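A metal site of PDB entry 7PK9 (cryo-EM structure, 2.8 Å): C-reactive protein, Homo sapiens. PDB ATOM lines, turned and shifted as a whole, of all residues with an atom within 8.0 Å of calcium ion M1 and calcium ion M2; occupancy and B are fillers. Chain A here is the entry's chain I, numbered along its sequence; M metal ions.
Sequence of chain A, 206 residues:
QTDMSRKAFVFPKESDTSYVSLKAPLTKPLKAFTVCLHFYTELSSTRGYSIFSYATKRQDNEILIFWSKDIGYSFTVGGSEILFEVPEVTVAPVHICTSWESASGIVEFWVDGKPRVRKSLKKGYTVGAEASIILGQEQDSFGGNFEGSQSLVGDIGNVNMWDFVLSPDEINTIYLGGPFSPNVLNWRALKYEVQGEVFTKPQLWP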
ATOM      1  N   SER A  50      -2.498  -9.196   1.148  1.00  0.00           N
ATOM      2  CA  SER A  50      -1.101  -9.397   1.493  1.00  0.00           C
ATOM      3  C   SER A  50      -0.463 -10.489   0.662  1.00  0.00           C
ATOM      4  O   SER A  50      -0.829 -11.663   0.785  1.00  0.00           O
ATOM      5  CB  SER A  50      -0.986  -9.712   2.977  1.00  0.00           C
ATOM      6  OG  SER A  50       0.352  -9.938   3.346  1.00  0.00           O
ATOM      7  N   SER A  53       4.206 -11.037   3.932  1.00  0.00           N
ATOM      8  CA  SER A  53       4.292 -10.315   5.201  1.00  0.00           C
ATOM      9  C   SER A  53       5.476 -10.797   6.036  1.00  0.00           C
ATOM     10  O   SER A  53       5.519 -11.953   6.457  1.00  0.00           O
ATOM     11  CB  SER A  53       2.995 -10.475   5.989  1.00  0.00           C
ATOM     12  OG  SER A  53       3.049  -9.700   7.163  1.00  0.00           O
ATOM     13  N   ALA A  55       7.265  -9.837   9.542  1.00  0.00           N
ATOM     14  CA  ALA A  55       7.031  -9.078  10.770  1.00  0.00           C
ATOM     15  C   ALA A  55       8.104  -9.333  11.825  1.00  0.00           C
ATOM     16  O   ALA A  55       8.719 -10.402  11.863  1.00  0.00           O
ATOM     17  CB  ALA A  55       5.673  -9.414  11.379  1.00  0.00           C
ATOM     18  N   GLN A  59       8.156  -4.084  14.746  1.00  0.00           N
ATOM     19  CA  GLN A  59       7.534  -3.586  13.524  1.00  0.00           C
ATOM     20  C   GLN A  59       6.821  -4.740  12.846  1.00  0.00           C
ATOM     21  O   GLN A  59       7.467  -5.721  12.473  1.00  0.00           O
ATOM     22  CB  GLN A  59       8.583  -2.967  12.597  1.00  0.00           C
ATOM     23  CG  GLN A  59       8.005  -2.343  11.368  1.00  0.00           C
ATOM     24  CD  GLN A  59       7.114  -1.182  11.704  1.00  0.00           C
ATOM     25  OE1 GLN A  59       5.895  -1.313  11.777  1.00  0.00           O
ATOM     26  NE2 GLN A  59       7.707  -0.023  11.918  1.00  0.00           N
ATOM     27  N   ASP A  60       5.491  -4.648  12.731  1.00  0.00           N
ATOM     28  CA  ASP A  60       4.723  -5.730  12.106  1.00  0.00           C
ATOM     29  C   ASP A  60       4.866  -5.752  10.590  1.00  0.00           C
ATOM     30  O   ASP A  60       4.870  -6.825   9.994  1.00  0.00           O
ATOM     31  CB  ASP A  60       3.252  -5.595  12.469  1.00  0.00           C
ATOM     32  CG  ASP A  60       2.654  -4.301  11.981  1.00  0.00           C
ATOM     33  OD1 ASP A  60       3.423  -3.330  11.828  1.00  0.00           O
ATOM     34  OD2 ASP A  60       1.435  -4.255  11.731  1.00  0.00           O
ATOM     35  N   ASN A  61       4.983  -4.589   9.953  1.00  0.00           N
ATOM     36  CA  ASN A  61       5.134  -4.489   8.505  1.00  0.00           C
ATOM     37  C   ASN A  61       6.594  -4.298   8.132  1.00  0.00           C
ATOM     38  O   ASN A  61       6.937  -3.404   7.366  1.00  0.00           O
ATOM     39  CB  ASN A  61       4.294  -3.344   7.978  1.00  0.00           C
ATOM     40  CG  ASN A  61       2.827  -3.544   8.212  1.00  0.00           C
ATOM     41  OD1 ASN A  61       2.395  -4.599   8.679  1.00  0.00           O
ATOM     42  ND2 ASN A  61       2.030  -2.541   7.884  1.00  0.00           N
ATOM     43  N   GLU A  62       7.472  -5.147   8.637  1.00  0.00           N
ATOM     44  CA  GLU A  62       8.890  -4.900   8.431  1.00  0.00           C
ATOM     45  C   GLU A  62       9.265  -5.077   6.965  1.00  0.00           C
ATOM     46  O   GLU A  62      10.119  -4.350   6.443  1.00  0.00           O
ATOM     47  CB  GLU A  62       9.710  -5.834   9.304  1.00  0.00           C
ATOM     48  CG  GLU A  62      11.194  -5.718   9.145  1.00  0.00           C
ATOM     49  CD  GLU A  62      11.750  -4.580   9.970  1.00  0.00           C
ATOM     50  OE1 GLU A  62      12.964  -4.544  10.182  1.00  0.00           O
ATOM     51  OE2 GLU A  62      10.956  -3.737  10.411  1.00  0.00           O
ATOM     52  N   LEU A  64       6.376  -5.598   3.744  1.00  0.00           N
ATOM     53  CA  LEU A  64       5.069  -5.963   3.194  1.00  0.00           C
ATOM     54  C   LEU A  64       5.060  -5.679   1.713  1.00  0.00           C
ATOM     55  O   LEU A  64       5.274  -4.535   1.303  1.00  0.00           O
ATOM     56  CB  LEU A  64       3.949  -5.204   3.900  1.00  0.00           C
ATOM     57  CG  LEU A  64       2.538  -5.719   3.638  1.00  0.00           C
ATOM     58  CD1 LEU A  64       2.318  -7.111   4.187  1.00  0.00           C
ATOM     59  CD2 LEU A  64       1.525  -4.751   4.201  1.00  0.00           C
ATOM     60  N   PHE A  66       2.158  -5.585  -0.749  1.00  0.00           N
ATOM     61  CA  PHE A  66       0.715  -5.512  -0.610  1.00  0.00           C
ATOM     62  C   PHE A  66       0.105  -5.009  -1.908  1.00  0.00           C
ATOM     63  O   PHE A  66       0.527  -3.967  -2.426  1.00  0.00           O
ATOM     64  CB  PHE A  66       0.322  -4.600   0.554  1.00  0.00           C
ATOM     65  CG  PHE A  66      -1.048  -4.859   1.095  1.00  0.00           C
ATOM     66  CD1 PHE A  66      -1.257  -5.828   2.043  1.00  0.00           C
ATOM     67  CD2 PHE A  66      -2.118  -4.096   0.674  1.00  0.00           C
ATOM     68  CE1 PHE A  66      -2.523  -6.056   2.556  1.00  0.00           C
ATOM     69  CE2 PHE A  66      -3.389  -4.319   1.180  1.00  0.00           C
ATOM     70  CZ  PHE A  66      -3.581  -5.302   2.119  1.00  0.00           C
ATOM     71  N   THR A  76       6.420  -1.911   1.344  1.00  0.00           N
ATOM     72  CA  THR A  76       6.828  -1.289   2.608  1.00  0.00           C
ATOM     73  C   THR A  76       8.058  -1.984   3.155  1.00  0.00           C
ATOM     74  O   THR A  76       8.176  -3.211   3.093  1.00  0.00           O
ATOM     75  CB  THR A  76       5.736  -1.354   3.702  1.00  0.00           C
ATOM     76  OG1 THR A  76       5.430  -2.663   4.214  1.00  0.00           O
ATOM     77  CG2 THR A  76       4.719  -0.225   3.810  1.00  0.00           C
ATOM     78  N   GLN A 137      -1.597 -14.169   4.775  1.00  0.00           N
ATOM     79  CA  GLN A 137      -2.196 -13.219   5.689  1.00  0.00           C
ATOM     80  C   GLN A 137      -1.329 -11.977   5.740  1.00  0.00           C
ATOM     81  O   GLN A 137      -0.116 -12.048   5.522  1.00  0.00           O
ATOM     82  CB  GLN A 137      -2.339 -13.801   7.089  1.00  0.00           C
ATOM     83  CG  GLN A 137      -3.192 -15.047   7.189  1.00  0.00           C
ATOM     84  CD  GLN A 137      -4.645 -14.782   6.951  1.00  0.00           C
ATOM     85  OE1 GLN A 137      -5.088 -13.642   7.004  1.00  0.00           O
ATOM     86  NE2 GLN A 137      -5.394 -15.824   6.682  1.00  0.00           N
ATOM     87  N   GLU A 138      -1.953 -10.849   6.033  1.00  0.00           N
ATOM     88  CA  GLU A 138      -1.224  -9.728   6.611  1.00  0.00           C
ATOM     89  C   GLU A 138      -1.239  -9.924   8.117  1.00  0.00           C
ATOM     90  O   GLU A 138      -2.249 -10.381   8.672  1.00  0.00           O
ATOM     91  CB  GLU A 138      -1.862  -8.401   6.222  1.00  0.00           C
ATOM     92  CG  GLU A 138      -0.898  -7.217   6.285  1.00  0.00           C
ATOM     93  CD  GLU A 138      -0.897  -6.527   7.630  1.00  0.00           C
ATOM     94  OE1 GLU A 138      -1.703  -6.887   8.507  1.00  0.00           O
ATOM     95  OE2 GLU A 138      -0.049  -5.626   7.813  1.00  0.00           O
ATOM     96  N   GLN A 139      -0.141  -9.585   8.771  1.00  0.00           N
ATOM     97  CA  GLN A 139      -0.026  -9.755  10.215  1.00  0.00           C
ATOM     98  C   GLN A 139       0.252  -8.429  10.897  1.00  0.00           C
ATOM     99  O   GLN A 139       0.894  -7.539  10.336  1.00  0.00           O
ATOM    100  CB  GLN A 139       1.060 -10.771  10.550  1.00  0.00           C
ATOM    101  CG  GLN A 139       2.462 -10.272  10.430  1.00  0.00           C
ATOM    102  CD  GLN A 139       3.436 -11.413  10.275  1.00  0.00           C
ATOM    103  OE1 GLN A 139       3.567 -12.253  11.157  1.00  0.00           O
ATOM    104  NE2 GLN A 139       4.147 -11.435   9.159  1.00  0.00           N
ATOM    105  N   ASP A 140      -0.261  -8.306  12.119  1.00  0.00           N
ATOM    106  CA  ASP A 140      -0.123  -7.085  12.913  1.00  0.00           C
ATOM    107  C   ASP A 140       0.487  -7.367  14.273  1.00  0.00           C
ATOM    108  O   ASP A 140       1.118  -6.492  14.864  1.00  0.00           O
ATOM    109  CB  ASP A 140      -1.494  -6.424  13.097  1.00  0.00           C
ATOM    110  CG  ASP A 140      -2.038  -5.877  11.820  1.00  0.00           C
ATOM    111  OD1 ASP A 140      -3.283  -5.854  11.682  1.00  0.00           O
ATOM    112  OD2 ASP A 140      -1.245  -5.466  10.954  1.00  0.00           O
ATOM    113  N   SER A 141       0.292  -8.570  14.795  1.00  0.00           N
ATOM    114  CA  SER A 141       1.085  -9.032  15.927  1.00  0.00           C
ATOM    115  C   SER A 141       2.423  -9.533  15.391  1.00  0.00           C
ATOM    116  O   SER A 141       2.747  -9.369  14.221  1.00  0.00           O
ATOM    117  CB  SER A 141       0.326 -10.092  16.719  1.00  0.00           C
ATOM    118  OG  SER A 141       0.410 -11.356  16.090  1.00  0.00           O
ATOM    119  N   GLY A 144       0.585 -12.952  14.078  1.00  0.00           N
ATOM    120  CA  GLY A 144      -0.836 -13.152  14.197  1.00  0.00           C
ATOM    121  C   GLY A 144      -1.588 -11.856  14.063  1.00  0.00           C
ATOM    122  O   GLY A 144      -1.108 -10.880  13.480  1.00  0.00           O
ATOM    123  N   ASN A 145      -2.795 -11.838  14.631  1.00  0.00           N
ATOM    124  CA  ASN A 145      -3.744 -10.744  14.444  1.00  0.00           C
ATOM    125  C   ASN A 145      -3.998 -10.498  12.957  1.00  0.00           C
ATOM    126  O   ASN A 145      -3.928  -9.375  12.456  1.00  0.00           O
ATOM    127  CB  ASN A 145      -3.229  -9.479  15.131  1.00  0.00           C
ATOM    128  CG  ASN A 145      -4.287  -8.394  15.219  1.00  0.00           C
ATOM    129  OD1 ASN A 145      -5.470  -8.645  14.993  1.00  0.00           O
ATOM    130  ND2 ASN A 145      -3.856  -7.183  15.543  1.00  0.00           N
ATOM    131  N   PHE A 146      -4.309 -11.578  12.244  1.00  0.00           N
ATOM    132  CA  PHE A 146      -4.630 -11.515  10.829  1.00  0.00           C
ATOM    133  C   PHE A 146      -5.993 -10.871  10.619  1.00  0.00           C
ATOM    134  O   PHE A 146      -6.805 -10.733  11.543  1.00  0.00           O
ATOM    135  CB  PHE A 146      -4.609 -12.899  10.194  1.00  0.00           C
ATOM    136  CG  PHE A 146      -3.397 -13.687  10.542  1.00  0.00           C
ATOM    137  CD1 PHE A 146      -2.130 -13.182  10.323  1.00  0.00           C
ATOM    138  CD2 PHE A 146      -3.513 -14.944  11.103  1.00  0.00           C
ATOM    139  CE1 PHE A 146      -1.023 -13.900  10.647  1.00  0.00           C
ATOM    140  CE2 PHE A 146      -2.393 -15.669  11.428  1.00  0.00           C
ATOM    141  CZ  PHE A 146      -1.154 -15.158  11.202  1.00  0.00           C
ATOM    142  N   GLU A 147      -6.259 -10.476   9.370  1.00  0.00           N
ATOM    143  CA  GLU A 147      -7.530  -9.891   8.980  1.00  0.00           C
ATOM    144  C   GLU A 147      -8.043 -10.627   7.754  1.00  0.00           C
ATOM    145  O   GLU A 147      -7.323 -10.792   6.766  1.00  0.00           O
ATOM    146  CB  GLU A 147      -7.367  -8.402   8.644  1.00  0.00           C
ATOM    147  CG  GLU A 147      -7.014  -7.537   9.842  1.00  0.00           C
ATOM    148  CD  GLU A 147      -6.682  -6.109   9.445  1.00  0.00           C
ATOM    149  OE1 GLU A 147      -5.658  -5.902   8.762  1.00  0.00           O
ATOM    150  OE2 GLU A 147      -7.450  -5.184   9.802  1.00  0.00           O
ATOM    151  N   SER A 149     -10.238  -9.711   5.509  1.00  0.00           N
ATOM    152  CA  SER A 149     -10.280  -8.826   4.351  1.00  0.00           C
ATOM    153  C   SER A 149      -8.930  -8.593   3.708  1.00  0.00           C
ATOM    154  O   SER A 149      -8.877  -7.932   2.656  1.00  0.00           O
ATOM    155  CB  SER A 149     -10.893  -7.492   4.760  1.00  0.00           C
ATOM    156  OG  SER A 149     -10.116  -6.877   5.783  1.00  0.00           O
ATOM    157  N   GLN A 150      -7.829  -9.082   4.284  1.00  0.00           N
ATOM    158  CA  GLN A 150      -6.519  -8.922   3.682  1.00  0.00           C
ATOM    159  C   GLN A 150      -5.820 -10.230   3.385  1.00  0.00           C
ATOM    160  O   GLN A 150      -4.753 -10.215   2.779  1.00  0.00           O
ATOM    161  CB  GLN A 150      -5.637  -8.077   4.613  1.00  0.00           C
ATOM    162  CG  GLN A 150      -6.171  -6.676   4.819  1.00  0.00           C
ATOM    163  CD  GLN A 150      -5.140  -5.725   5.336  1.00  0.00           C
ATOM    164  OE1 GLN A 150      -4.171  -6.133   5.973  1.00  0.00           O
ATOM    165  NE2 GLN A 150      -5.330  -4.443   5.057  1.00  0.00           N
HETATM  166 CA    CA M   1      -3.394  -5.558   9.299  1.00  0.00          CA
HETATM  167 CA    CA M   2       0.310  -4.440   9.568  1.00  0.00          CA
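O of Gln 150 lies within hydrogen-bond range of N of Ser 50 (3.0 Å). The side-chain carboxylate (OD1) of Asp 60 sits close to the side-chain amide oxygen (OE1) of Gln 59. The side-chain amide nitrogen (NE2) of Gln 139 is in hydrogen-bond range of the side-chain hydroxyl (OG) of Ser 53, at 2.9 Å. OE1 of Glu 147 sits close to OE1 of Gln 150 (3.2 Å).
Gln 150 touches calcium ion M1. The nearest printed residue that does not touch calcium ion M1 is Gln 139 (4.8 Å).
Merely in contact with calcium ion M2: Gln 139 (3.2 Å). Of the 21 residues printed, 5 come within 4 Å of calcium ion M2. The nearest printed residue that does not touch calcium ion M2 is Leu 64 (5.5 Å).
Calcium ion M1 is bound by OE1 of Glu 138 (2.3 Å), OE1 of Glu 147 (2.4 Å), OD1 of Asp 140 (2.4 Å) and OD2 of Asp 140 (2.7 Å).
Calcium ion M2 is bound by the side-chain carboxylate (OE2) of Glu 138 (2.1 Å), the side-chain amide oxygen (OD1) of Asn 61 (2.3 Å), the side-chain carboxylate (OD2) of Asp 140 (2.3 Å) and the side-chain carboxylate (OD2) of Asp 60 (2.4 Å). Calcium ion M2 has four donor atoms within binding distance. Slightly farther from calcium ion M2 lies ND2 of Asn 61 (3.1 Å).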
